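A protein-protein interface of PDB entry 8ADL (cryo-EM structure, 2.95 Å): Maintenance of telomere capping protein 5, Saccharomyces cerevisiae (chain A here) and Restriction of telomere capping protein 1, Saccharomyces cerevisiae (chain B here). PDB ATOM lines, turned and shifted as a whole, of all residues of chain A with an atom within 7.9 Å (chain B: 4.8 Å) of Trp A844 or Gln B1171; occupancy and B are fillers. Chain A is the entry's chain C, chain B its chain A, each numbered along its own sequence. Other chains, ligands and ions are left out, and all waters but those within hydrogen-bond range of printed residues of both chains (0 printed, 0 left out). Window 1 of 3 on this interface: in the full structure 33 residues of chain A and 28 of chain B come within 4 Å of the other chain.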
ATOM      1  N   ILE A 826      26.133  -1.266  25.300  1.00  0.00           N
ATOM      2  CA  ILE A 826      24.770  -0.905  25.681  1.00  0.00           C
ATOM      3  C   ILE A 826      23.781  -1.318  24.595  1.00  0.00           C
ATOM      4  O   ILE A 826      22.694  -1.838  24.891  1.00  0.00           O
ATOM      5  CB  ILE A 826      24.702   0.601  25.997  1.00  0.00           C
ATOM      6  CG1 ILE A 826      25.405   0.895  27.323  1.00  0.00           C
ATOM      7  CG2 ILE A 826      23.276   1.094  26.056  1.00  0.00           C
ATOM      8  CD1 ILE A 826      24.842   0.130  28.496  1.00  0.00           C
ATOM      9  N   LEU A 827      24.149  -1.131  23.323  1.00  0.00           N
ATOM     10  CA  LEU A 827      23.287  -1.589  22.237  1.00  0.00           C
ATOM     11  C   LEU A 827      23.185  -3.113  22.200  1.00  0.00           C
ATOM     12  O   LEU A 827      22.123  -3.654  21.867  1.00  0.00           O
ATOM     13  CB  LEU A 827      23.805  -1.051  20.904  1.00  0.00           C
ATOM     14  CG  LEU A 827      22.846  -1.083  19.715  1.00  0.00           C
ATOM     15  CD1 LEU A 827      21.514  -0.458  20.085  1.00  0.00           C
ATOM     16  CD2 LEU A 827      23.457  -0.375  18.519  1.00  0.00           C
ATOM     17  N   ASP A 829      23.288  -5.020  24.908  1.00  0.00           N
ATOM     18  CA  ASP A 829      22.335  -5.314  25.976  1.00  0.00           C
ATOM     19  C   ASP A 829      20.904  -5.049  25.529  1.00  0.00           C
ATOM     20  O   ASP A 829      19.990  -5.809  25.866  1.00  0.00           O
ATOM     21  CB  ASP A 829      22.655  -4.487  27.218  1.00  0.00           C
ATOM     22  CG  ASP A 829      24.082  -4.643  27.670  1.00  0.00           C
ATOM     23  OD1 ASP A 829      24.641  -5.749  27.517  1.00  0.00           O
ATOM     24  OD2 ASP A 829      24.651  -3.647  28.158  1.00  0.00           O
ATOM     25  N   MET A 830      20.692  -3.974  24.769  1.00  0.00           N
ATOM     26  CA  MET A 830      19.346  -3.644  24.320  1.00  0.00           C
ATOM     27  C   MET A 830      18.857  -4.543  23.191  1.00  0.00           C
ATOM     28  O   MET A 830      17.652  -4.568  22.920  1.00  0.00           O
ATOM     29  CB  MET A 830      19.276  -2.183  23.876  1.00  0.00           C
ATOM     30  CG  MET A 830      18.958  -1.219  25.003  1.00  0.00           C
ATOM     31  SD  MET A 830      18.893   0.491  24.453  1.00  0.00           S
ATOM     32  CE  MET A 830      20.432   0.581  23.552  1.00  0.00           C
ATOM     33  N   LEU A 831      19.750  -5.278  22.526  1.00  0.00           N
ATOM     34  CA  LEU A 831      19.357  -6.167  21.439  1.00  0.00           C
ATOM     35  C   LEU A 831      19.456  -7.643  21.819  1.00  0.00           C
ATOM     36  O   LEU A 831      19.662  -8.497  20.953  1.00  0.00           O
ATOM     37  CB  LEU A 831      20.189  -5.887  20.189  1.00  0.00           C
ATOM     38  CG  LEU A 831      19.969  -4.533  19.511  1.00  0.00           C
ATOM     39  CD1 LEU A 831      21.120  -4.212  18.573  1.00  0.00           C
ATOM     40  CD2 LEU A 831      18.647  -4.505  18.769  1.00  0.00           C
ATOM     41  N   ILE A 832      19.309  -7.964  23.102  1.00  0.00           N
ATOM     42  CA  ILE A 832      19.377  -9.352  23.554  1.00  0.00           C
ATOM     43  C   ILE A 832      18.047 -10.036  23.265  1.00  0.00           C
ATOM     44  O   ILE A 832      16.983  -9.541  23.655  1.00  0.00           O
ATOM     45  CB  ILE A 832      19.721  -9.429  25.051  1.00  0.00           C
ATOM     46  CG1 ILE A 832      21.168  -9.015  25.301  1.00  0.00           C
ATOM     47  CG2 ILE A 832      19.479 -10.832  25.596  1.00  0.00           C
ATOM     48  CD1 ILE A 832      21.583  -9.073  26.753  1.00  0.00           C
ATOM     49  N   ASP A 838       8.596 -14.110  23.775  1.00  0.00           N
ATOM     50  CA  ASP A 838       7.669 -13.398  24.634  1.00  0.00           C
ATOM     51  C   ASP A 838       7.315 -12.032  24.046  1.00  0.00           C
ATOM     52  O   ASP A 838       8.168 -11.372  23.444  1.00  0.00           O
ATOM     53  CB  ASP A 838       8.227 -13.255  26.069  1.00  0.00           C
ATOM     54  CG  ASP A 838       9.594 -12.592  26.123  1.00  0.00           C
ATOM     55  OD1 ASP A 838      10.202 -12.332  25.067  1.00  0.00           O
ATOM     56  OD2 ASP A 838      10.068 -12.328  27.248  1.00  0.00           O
ATOM     57  N   PRO A 839       6.050 -11.611  24.151  1.00  0.00           N
ATOM     58  CA  PRO A 839       5.635 -10.365  23.485  1.00  0.00           C
ATOM     59  C   PRO A 839       6.175  -9.112  24.143  1.00  0.00           C
ATOM     60  O   PRO A 839       6.294  -8.080  23.465  1.00  0.00           O
ATOM     61  CB  PRO A 839       4.104 -10.408  23.580  1.00  0.00           C
ATOM     62  CG  PRO A 839       3.769 -11.813  23.958  1.00  0.00           C
ATOM     63  CD  PRO A 839       4.911 -12.297  24.776  1.00  0.00           C
ATOM     64  N   TYR A 840       6.497  -9.167  25.438  1.00  0.00           N
ATOM     65  CA  TYR A 840       6.898  -7.965  26.158  1.00  0.00           C
ATOM     66  C   TYR A 840       8.256  -7.458  25.698  1.00  0.00           C
ATOM     67  O   TYR A 840       8.515  -6.252  25.766  1.00  0.00           O
ATOM     68  CB  TYR A 840       6.897  -8.231  27.663  1.00  0.00           C
ATOM     69  CG  TYR A 840       5.535  -8.604  28.200  1.00  0.00           C
ATOM     70  CD1 TYR A 840       4.479  -7.703  28.145  1.00  0.00           C
ATOM     71  CD2 TYR A 840       5.302  -9.856  28.756  1.00  0.00           C
ATOM     72  CE1 TYR A 840       3.229  -8.036  28.631  1.00  0.00           C
ATOM     73  CE2 TYR A 840       4.055 -10.198  29.245  1.00  0.00           C
ATOM     74  CZ  TYR A 840       3.024  -9.284  29.179  1.00  0.00           C
ATOM     75  OH  TYR A 840       1.781  -9.619  29.664  1.00  0.00           O
ATOM     76  N   THR A 841       9.118  -8.348  25.197  1.00  0.00           N
ATOM     77  CA  THR A 841      10.362  -7.902  24.577  1.00  0.00           C
ATOM     78  C   THR A 841      10.094  -7.085  23.320  1.00  0.00           C
ATOM     79  O   THR A 841      10.736  -6.053  23.101  1.00  0.00           O
ATOM     80  CB  THR A 841      11.256  -9.096  24.253  1.00  0.00           C
ATOM     81  OG1 THR A 841      10.468 -10.148  23.681  1.00  0.00           O
ATOM     82  CG2 THR A 841      11.943  -9.591  25.508  1.00  0.00           C
ATOM     83  N   THR A 842       9.138  -7.516  22.493  1.00  0.00           N
ATOM     84  CA  THR A 842       8.792  -6.754  21.294  1.00  0.00           C
ATOM     85  C   THR A 842       8.142  -5.423  21.655  1.00  0.00           C
ATOM     86  O   THR A 842       8.417  -4.396  21.015  1.00  0.00           O
ATOM     87  CB  THR A 842       7.870  -7.579  20.396  1.00  0.00           C
ATOM     88  OG1 THR A 842       8.414  -8.894  20.229  1.00  0.00           O
ATOM     89  CG2 THR A 842       7.730  -6.927  19.030  1.00  0.00           C
ATOM     90  N   ILE A 843       7.289  -5.422  22.685  1.00  0.00           N
ATOM     91  CA  ILE A 843       6.644  -4.188  23.131  1.00  0.00           C
ATOM     92  C   ILE A 843       7.679  -3.207  23.676  1.00  0.00           C
ATOM     93  O   ILE A 843       7.614  -2.001  23.408  1.00  0.00           O
ATOM     94  CB  ILE A 843       5.549  -4.509  24.166  1.00  0.00           C
ATOM     95  CG1 ILE A 843       4.461  -5.376  23.534  1.00  0.00           C
ATOM     96  CG2 ILE A 843       4.926  -3.238  24.719  1.00  0.00           C
ATOM     97  CD1 ILE A 843       3.638  -6.146  24.538  1.00  0.00           C
ATOM     98  N   TRP A 844       8.661  -3.710  24.429  1.00  0.00           N
ATOM     99  CA  TRP A 844       9.725  -2.857  24.945  1.00  0.00           C
ATOM    100  C   TRP A 844      10.654  -2.372  23.840  1.00  0.00           C
ATOM    101  O   TRP A 844      11.175  -1.253  23.919  1.00  0.00           O
ATOM    102  CB  TRP A 844      10.520  -3.608  26.009  1.00  0.00           C
ATOM    103  CG  TRP A 844      11.603  -2.799  26.626  1.00  0.00           C
ATOM    104  CD1 TRP A 844      11.482  -1.903  27.643  1.00  0.00           C
ATOM    105  CD2 TRP A 844      12.986  -2.813  26.264  1.00  0.00           C
ATOM    106  NE1 TRP A 844      12.707  -1.354  27.937  1.00  0.00           N
ATOM    107  CE2 TRP A 844      13.646  -1.897  27.102  1.00  0.00           C
ATOM    108  CE3 TRP A 844      13.730  -3.510  25.310  1.00  0.00           C
ATOM    109  CZ2 TRP A 844      15.014  -1.660  27.015  1.00  0.00           C
ATOM    110  CZ3 TRP A 844      15.087  -3.275  25.227  1.00  0.00           C
ATOM    111  CH2 TRP A 844      15.715  -2.359  26.074  1.00  0.00           C
ATOM    112  N   ASN A 845      10.890  -3.202  22.821  1.00  0.00           N
ATOM    113  CA  ASN A 845      11.710  -2.788  21.689  1.00  0.00           C
ATOM    114  C   ASN A 845      11.043  -1.665  20.907  1.00  0.00           C
ATOM    115  O   ASN A 845      11.692  -0.671  20.563  1.00  0.00           O
ATOM    116  CB  ASN A 845      11.983  -3.982  20.775  1.00  0.00           C
ATOM    117  CG  ASN A 845      13.010  -4.934  21.350  1.00  0.00           C
ATOM    118  OD1 ASN A 845      13.707  -4.610  22.309  1.00  0.00           O
ATOM    119  ND2 ASN A 845      13.100  -6.125  20.771  1.00  0.00           N
ATOM    120  N   ASN A 846       9.744  -1.790  20.642  1.00  0.00           N
ATOM    121  CA  ASN A 846       9.035  -0.788  19.856  1.00  0.00           C
ATOM    122  C   ASN A 846       8.725   0.491  20.628  1.00  0.00           C
ATOM    123  O   ASN A 846       8.169   1.422  20.036  1.00  0.00           O
ATOM    124  CB  ASN A 846       7.736  -1.382  19.307  1.00  0.00           C
ATOM    125  CG  ASN A 846       7.982  -2.537  18.359  1.00  0.00           C
ATOM    126  OD1 ASN A 846       9.051  -2.643  17.757  1.00  0.00           O
ATOM    127  ND2 ASN A 846       6.993  -3.411  18.222  1.00  0.00           N
ATOM    128  N   HIS A 847       9.046   0.558  21.918  1.00  0.00           N
ATOM    129  CA  HIS A 847       8.782   1.767  22.688  1.00  0.00           C
ATOM    130  C   HIS A 847       9.720   2.890  22.245  1.00  0.00           C
ATOM    131  O   HIS A 847      10.884   2.636  21.921  1.00  0.00           O
ATOM    132  CB  HIS A 847       8.948   1.498  24.183  1.00  0.00           C
ATOM    133  CG  HIS A 847       8.088   2.363  25.049  1.00  0.00           C
ATOM    134  ND1 HIS A 847       8.540   3.533  25.618  1.00  0.00           N
ATOM    135  CD2 HIS A 847       6.797   2.232  25.436  1.00  0.00           C
ATOM    136  CE1 HIS A 847       7.568   4.085  26.321  1.00  0.00           C
ATOM    137  NE2 HIS A 847       6.499   3.315  26.226  1.00  0.00           N
ATOM    138  N   PRO A 848       9.240   4.137  22.205  1.00  0.00           N
ATOM    139  CA  PRO A 848      10.113   5.246  21.783  1.00  0.00           C
ATOM    140  C   PRO A 848      11.226   5.571  22.763  1.00  0.00           C
ATOM    141  O   PRO A 848      12.276   6.069  22.338  1.00  0.00           O
ATOM    142  CB  PRO A 848       9.138   6.424  21.640  1.00  0.00           C
ATOM    143  CG  PRO A 848       7.802   5.797  21.474  1.00  0.00           C
ATOM    144  CD  PRO A 848       7.836   4.560  22.313  1.00  0.00           C
ATOM    145  N   MET A 849      11.041   5.308  24.053  1.00  0.00           N
ATOM    146  CA  MET A 849      12.027   5.685  25.057  1.00  0.00           C
ATOM    147  C   MET A 849      13.135   4.656  25.225  1.00  0.00           C
ATOM    148  O   MET A 849      14.095   4.918  25.957  1.00  0.00           O
ATOM    149  CB  MET A 849      11.340   5.928  26.405  1.00  0.00           C
ATOM    150  CG  MET A 849      10.009   6.650  26.288  1.00  0.00           C
ATOM    151  SD  MET A 849       9.250   6.995  27.883  1.00  0.00           S
ATOM    152  CE  MET A 849      10.230   8.394  28.418  1.00  0.00           C
ATOM    153  N   GLY A 850      13.026   3.502  24.577  1.00  0.00           N
ATOM    154  CA  GLY A 850      14.086   2.516  24.574  1.00  0.00           C
ATOM    155  C   GLY A 850      14.536   2.240  23.153  1.00  0.00           C
ATOM    156  O   GLY A 850      13.758   2.369  22.206  1.00  0.00           O
ATOM    157  N   ILE A 851      15.819   1.889  23.013  1.00  0.00           N
ATOM    158  CA  ILE A 851      16.506   1.616  21.747  1.00  0.00           C
ATOM    159  C   ILE A 851      16.482   2.815  20.802  1.00  0.00           C
ATOM    160  O   ILE A 851      17.540   3.358  20.466  1.00  0.00           O
ATOM    161  CB  ILE A 851      15.941   0.364  21.050  1.00  0.00           C
ATOM    162  CG1 ILE A 851      16.085  -0.858  21.957  1.00  0.00           C
ATOM    163  CG2 ILE A 851      16.647   0.137  19.724  1.00  0.00           C
ATOM    164  CD1 ILE A 851      15.669  -2.156  21.309  1.00  0.00           C
ATOM    165  N   LYS A 852      15.286   3.222  20.358  1.00  0.00           N
ATOM    166  CA  LYS A 852      15.159   4.324  19.403  1.00  0.00           C
ATOM    167  C   LYS A 852      15.684   5.635  19.979  1.00  0.00           C
ATOM    168  O   LYS A 852      16.343   6.411  19.274  1.00  0.00           O
ATOM    169  CB  LYS A 852      13.701   4.473  18.976  1.00  0.00           C
ATOM    170  CG  LYS A 852      13.098   3.216  18.381  1.00  0.00           C
ATOM    171  CD  LYS A 852      11.696   3.475  17.864  1.00  0.00           C
ATOM    172  CE  LYS A 852      11.078   2.213  17.289  1.00  0.00           C
ATOM    173  NZ  LYS A 852       9.714   2.465  16.749  1.00  0.00           N
ATOM    174  N   ALA A1009       2.285  -7.658  18.900  1.00  0.00           N
ATOM    175  CA  ALA A1009       3.639  -8.195  18.986  1.00  0.00           C
ATOM    176  C   ALA A1009       3.723  -9.574  18.344  1.00  0.00           C
ATOM    177  O   ALA A1009       4.733  -9.911  17.714  1.00  0.00           O
ATOM    178  CB  ALA A1009       4.092  -8.250  20.444  1.00  0.00           C
ATOM    179  N   LEU A1015      12.195  -7.497  14.833  1.00  0.00           N
ATOM    180  CA  LEU A1015      12.628  -7.152  16.183  1.00  0.00           C
ATOM    181  C   LEU A1015      12.232  -5.722  16.537  1.00  0.00           C
ATOM    182  O   LEU A1015      11.809  -5.449  17.666  1.00  0.00           O
ATOM    183  CB  LEU A1015      14.141  -7.348  16.298  1.00  0.00           C
ATOM    184  CG  LEU A1015      14.905  -7.383  17.627  1.00  0.00           C
ATOM    185  CD1 LEU A1015      16.164  -8.208  17.439  1.00  0.00           C
ATOM    186  CD2 LEU A1015      15.276  -6.005  18.140  1.00  0.00           C
ATOM    187  N   LEU A1016      12.365  -4.801  15.586  1.00  0.00           N
ATOM    188  CA  LEU A1016      12.011  -3.402  15.772  1.00  0.00           C
ATOM    189  C   LEU A1016      11.135  -2.933  14.622  1.00  0.00           C
ATOM    190  O   LEU A1016      11.283  -3.388  13.485  1.00  0.00           O
ATOM    191  CB  LEU A1016      13.259  -2.515  15.851  1.00  0.00           C
ATOM    192  CG  LEU A1016      14.114  -2.628  17.108  1.00  0.00           C
ATOM    193  CD1 LEU A1016      15.578  -2.456  16.768  1.00  0.00           C
ATOM    194  CD2 LEU A1016      13.687  -1.591  18.120  1.00  0.00           C
ATOM    195  N   THR B 868      12.379  -8.857  29.234  1.00  0.00           N
ATOM    196  CA  THR B 868      12.217  -7.416  29.048  1.00  0.00           C
ATOM    197  C   THR B 868      12.732  -6.591  30.221  1.00  0.00           C
ATOM    198  O   THR B 868      13.002  -5.399  30.042  1.00  0.00           O
ATOM    199  CB  THR B 868      10.744  -7.088  28.790  1.00  0.00           C
ATOM    200  OG1 THR B 868      10.605  -5.686  28.527  1.00  0.00           O
ATOM    201  CG2 THR B 868       9.873  -7.477  29.978  1.00  0.00           C
ATOM    202  N   LYS B 871      16.948  -7.457  30.542  1.00  0.00           N
ATOM    203  CA  LYS B 871      17.706  -6.526  29.709  1.00  0.00           C
ATOM    204  C   LYS B 871      17.904  -5.189  30.415  1.00  0.00           C
ATOM    205  O   LYS B 871      18.984  -4.591  30.329  1.00  0.00           O
ATOM    206  CB  LYS B 871      17.000  -6.330  28.368  1.00  0.00           C
ATOM    207  CG  LYS B 871      17.073  -7.537  27.450  1.00  0.00           C
ATOM    208  CD  LYS B 871      16.896  -7.146  25.994  1.00  0.00           C
ATOM    209  CE  LYS B 871      15.427  -7.013  25.633  1.00  0.00           C
ATOM    210  NZ  LYS B 871      15.235  -6.574  24.224  1.00  0.00           N
ATOM    211  N   ILE B 872      16.877  -4.720  31.135  1.00  0.00           N
ATOM    212  CA  ILE B 872      16.962  -3.449  31.854  1.00  0.00           C
ATOM    213  C   ILE B 872      18.030  -3.524  32.937  1.00  0.00           C
ATOM    214  O   ILE B 872      18.875  -2.627  33.071  1.00  0.00           O
ATOM    215  CB  ILE B 872      15.592  -3.080  32.450  1.00  0.00           C
ATOM    216  CG1 ILE B 872      14.572  -2.816  31.345  1.00  0.00           C
ATOM    217  CG2 ILE B 872      15.707  -1.877  33.375  1.00  0.00           C
ATOM    218  CD1 ILE B 872      14.826  -1.547  30.585  1.00  0.00           C
ATOM    219  N   LEU B 875      21.497  -3.610  31.479  1.00  0.00           N
ATOM    220  CA  LEU B 875      21.889  -2.249  31.117  1.00  0.00           C
ATOM    221  C   LEU B 875      22.335  -1.453  32.338  1.00  0.00           C
ATOM    222  O   LEU B 875      23.346  -0.740  32.290  1.00  0.00           O
ATOM    223  CB  LEU B 875      20.723  -1.537  30.432  1.00  0.00           C
ATOM    224  CG  LEU B 875      20.347  -1.921  29.003  1.00  0.00           C
ATOM    225  CD1 LEU B 875      18.883  -1.615  28.747  1.00  0.00           C
ATOM    226  CD2 LEU B 875      21.214  -1.181  28.025  1.00  0.00           C
ATOM    227  N   GLN B1167      16.352   7.478  32.092  1.00  0.00           N
ATOM    228  CA  GLN B1167      15.504   7.144  30.951  1.00  0.00           C
ATOM    229  C   GLN B1167      14.825   5.792  31.137  1.00  0.00           C
ATOM    230  O   GLN B1167      13.657   5.623  30.761  1.00  0.00           O
ATOM    231  CB  GLN B1167      16.326   7.166  29.664  1.00  0.00           C
ATOM    232  CG  GLN B1167      15.493   7.057  28.403  1.00  0.00           C
ATOM    233  CD  GLN B1167      14.642   8.287  28.157  1.00  0.00           C
ATOM    234  OE1 GLN B1167      13.523   8.190  27.655  1.00  0.00           O
ATOM    235  NE2 GLN B1167      15.172   9.455  28.506  1.00  0.00           N
ATOM    236  N   LEU B1168      15.534   4.817  31.715  1.00  0.00           N
ATOM    237  CA  LEU B1168      14.905   3.539  32.034  1.00  0.00           C
ATOM    238  C   LEU B1168      13.834   3.710  33.105  1.00  0.00           C
ATOM    239  O   LEU B1168      12.786   3.056  33.050  1.00  0.00           O
ATOM    240  CB  LEU B1168      15.955   2.517  32.470  1.00  0.00           C
ATOM    241  CG  LEU B1168      16.983   2.100  31.416  1.00  0.00           C
ATOM    242  CD1 LEU B1168      17.787   0.900  31.885  1.00  0.00           C
ATOM    243  CD2 LEU B1168      16.323   1.823  30.074  1.00  0.00           C
ATOM    244  N   TYR B1169      14.079   4.601  34.073  1.00  0.00           N
ATOM    245  CA  TYR B1169      13.067   4.946  35.069  1.00  0.00           C
ATOM    246  C   TYR B1169      11.831   5.550  34.414  1.00  0.00           C
ATOM    247  O   TYR B1169      10.699   5.216  34.783  1.00  0.00           O
ATOM    248  CB  TYR B1169      13.680   5.913  36.090  1.00  0.00           C
ATOM    249  CG  TYR B1169      12.719   6.681  36.985  1.00  0.00           C
ATOM    250  CD1 TYR B1169      12.215   7.924  36.604  1.00  0.00           C
ATOM    251  CD2 TYR B1169      12.355   6.188  38.229  1.00  0.00           C
ATOM    252  CE1 TYR B1169      11.348   8.623  37.413  1.00  0.00           C
ATOM    253  CE2 TYR B1169      11.495   6.894  39.052  1.00  0.00           C
ATOM    254  CZ  TYR B1169      10.994   8.106  38.638  1.00  0.00           C
ATOM    255  OH  TYR B1169      10.138   8.809  39.452  1.00  0.00           O
ATOM    256  N   ASN B1170      12.032   6.458  33.456  1.00  0.00           N
ATOM    257  CA  ASN B1170      10.904   7.117  32.808  1.00  0.00           C
ATOM    258  C   ASN B1170      10.112   6.144  31.942  1.00  0.00           C
ATOM    259  O   ASN B1170       8.877   6.193  31.916  1.00  0.00           O
ATOM    260  CB  ASN B1170      11.398   8.297  31.973  1.00  0.00           C
ATOM    261  CG  ASN B1170      11.827   9.470  32.824  1.00  0.00           C
ATOM    262  OD1 ASN B1170      11.388   9.618  33.963  1.00  0.00           O
ATOM    263  ND2 ASN B1170      12.696  10.311  32.276  1.00  0.00           N
ATOM    264  N   GLN B1171      10.806   5.236  31.250  1.00  0.00           N
ATOM    265  CA  GLN B1171      10.114   4.201  30.487  1.00  0.00           C
ATOM    266  C   GLN B1171       9.352   3.247  31.400  1.00  0.00           C
ATOM    267  O   GLN B1171       8.248   2.806  31.058  1.00  0.00           O
ATOM    268  CB  GLN B1171      11.112   3.433  29.623  1.00  0.00           C
ATOM    269  CG  GLN B1171      10.465   2.550  28.576  1.00  0.00           C
ATOM    270  CD  GLN B1171      11.439   1.565  27.972  1.00  0.00           C
ATOM    271  OE1 GLN B1171      12.342   1.075  28.648  1.00  0.00           O
ATOM    272  NE2 GLN B1171      11.262   1.268  26.691  1.00  0.00           N
ATOM    273  N   ALA B1172       9.922   2.923  32.565  1.00  0.00           N
ATOM    274  CA  ALA B1172       9.232   2.061  33.518  1.00  0.00           C
ATOM    275  C   ALA B1172       7.989   2.731  34.087  1.00  0.00           C
ATOM    276  O   ALA B1172       6.936   2.094  34.208  1.00  0.00           O
ATOM    277  CB  ALA B1172      10.183   1.661  34.645  1.00  0.00           C
ATOM    278  N   THR B1173       8.084   4.012  34.441  1.00  0.00           N
ATOM    279  CA  THR B1173       6.937   4.697  35.020  1.00  0.00           C
ATOM    280  C   THR B1173       5.925   5.141  33.973  1.00  0.00           C
ATOM    281  O   THR B1173       4.808   5.520  34.341  1.00  0.00           O
ATOM    282  CB  THR B1173       7.389   5.901  35.850  1.00  0.00           C
ATOM    283  OG1 THR B1173       6.279   6.390  36.611  1.00  0.00           O
ATOM    284  CG2 THR B1173       7.884   7.016  34.959  1.00  0.00           C
ATOM    285  N   GLU B1174       6.279   5.109  32.687  1.00  0.00           N
ATOM    286  CA  GLU B1174       5.287   5.311  31.637  1.00  0.00           C
ATOM    287  C   GLU B1174       4.607   4.007  31.244  1.00  0.00           C
ATOM    288  O   GLU B1174       3.416   4.006  30.917  1.00  0.00           O
ATOM    289  CB  GLU B1174       5.933   5.958  30.410  1.00  0.00           C
ATOM    290  CG  GLU B1174       6.122   7.458  30.538  1.00  0.00           C
ATOM    291  CD  GLU B1174       4.901   8.236  30.096  1.00  0.00           C
ATOM    292  OE1 GLU B1174       4.161   7.737  29.223  1.00  0.00           O
ATOM    293  OE2 GLU B1174       4.680   9.347  30.623  1.00  0.00           O
ATOM    294  N   THR B1175       5.344   2.894  31.259  1.00  0.00           N
ATOM    295  CA  THR B1175       4.752   1.609  30.906  1.00  0.00           C
ATOM    296  C   THR B1175       3.822   1.118  32.008  1.00  0.00           C
ATOM    297  O   THR B1175       2.707   0.659  31.736  1.00  0.00           O
ATOM    298  CB  THR B1175       5.850   0.582  30.629  1.00  0.00           C
ATOM    299  OG1 THR B1175       6.823   1.148  29.743  1.00  0.00           O
ATOM    300  CG2 THR B1175       5.260  -0.669  29.993  1.00  0.00           C
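Hydrophobic or aromatic side chains of chain A within 4 Å of the printed part of chain B: Ile A826, Met A830, Ile A832, Tyr A840, Trp A844, His A847 and Met A849.
Along chain A the printed residues that touch a printed residue of chain B span positions 826 to 850.
Of the 13 printed residues of chain B, 7 touch a printed residue of chain A.
Hydrophobic or aromatic side chains of chain B that line the printed part of chain A: Ile B872 and Leu B875.
Among the printed residues, no Asp or Glu carboxylate lies within 4 Å of a Lys or Arg side-chain nitrogen of the other chain.
The side-chain amide nitrogen (ND2) of Asn A845 lies close to the backbone carbonyl oxygen (O) of Leu A1015 (3.4 Å).
SD of Met A830 lies within hydrogen-bond range of N of Ile A851, at 3.7 Å.
N of Met A849 sits close to ND1 of His A847 (3.4 Å).
O of Thr A841 sits close to ND2 of Asn A845, 3.3 Å away.
The side-chain carboxylate (OD1) of Asp A838 sits at hydrogen-bond distance from the side-chain hydroxyl (OG1) of Thr A841 (2.6 Å).
The side-chain hydroxyl (OG1) of Thr B1175 is in hydrogen-bond range of the backbone carbonyl oxygen (O) of Gln B1171 (2.6 Å).
Ile A826 touches Leu B875.
CD2 of Leu B875 touches CB of Asp A829, at 3.7 Å.
CG of Met A830 touches CD1 of Leu B875 (3.8 Å).
O of Tyr A840 touches OG1 of Thr B868, at 3.5 Å.
Thr A841 touches Thr B868.
Trp A844 touches Thr B868 (CB to OG1, 3.3 Å).
CB of Met A849 touches OE1 of Gln B1167 (3.4 Å).
Asn B1170 touches Met A849.
Met A849 touches Gln B1171.
Gly A850 touches Gln B1171.
Trp A844 touches just these residues of chain B: Thr B868 (3.3 Å), Lys B871 (3.5 Å), Ile B872 (3.4 Å) and Gln B1171 (2.6 Å).
Ala B1172 touches none of the printed residues of chain A.
Printed residues of chain A within 4 Å of Asn B1170: Met A849 (3.7 Å).
Printed residues of chain A within 4 Å of Thr B868: Tyr A840, Thr A841 and Trp A844.
Printed residues of chain B within 4 Å of Ile A826: Leu B875.
Pro A848 touches none of the printed residues of chain B.
Ile A843 touches none of the printed residues of chain B.
The nearest residue of chain B that does not touch Trp A844 is Leu B875 (4.2 Å).
The nearest residue of chain A that does not touch Gln B1171 is Pro A848 (5.7 Å).
The backbone carbonyl oxygen (O) of Ile A832 lies close to the side-chain amino group (NZ) of Lys B871, at 3.5 Å.
The side-chain amino group of Lys B871 lies within hydrogen-bond range of the backbone carbonyl oxygen of Met A830, at 3.4 Å.
The side-chain amide oxygen (OD1) of Asn A845 sits at hydrogen-bond distance from the side-chain amino group (NZ) of Lys B871 (3.1 Å).
The indole nitrogen (NE1) of Trp A844 is in hydrogen-bond range of the side-chain amide oxygen (OE1) of Gln B1171 (2.6 Å).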
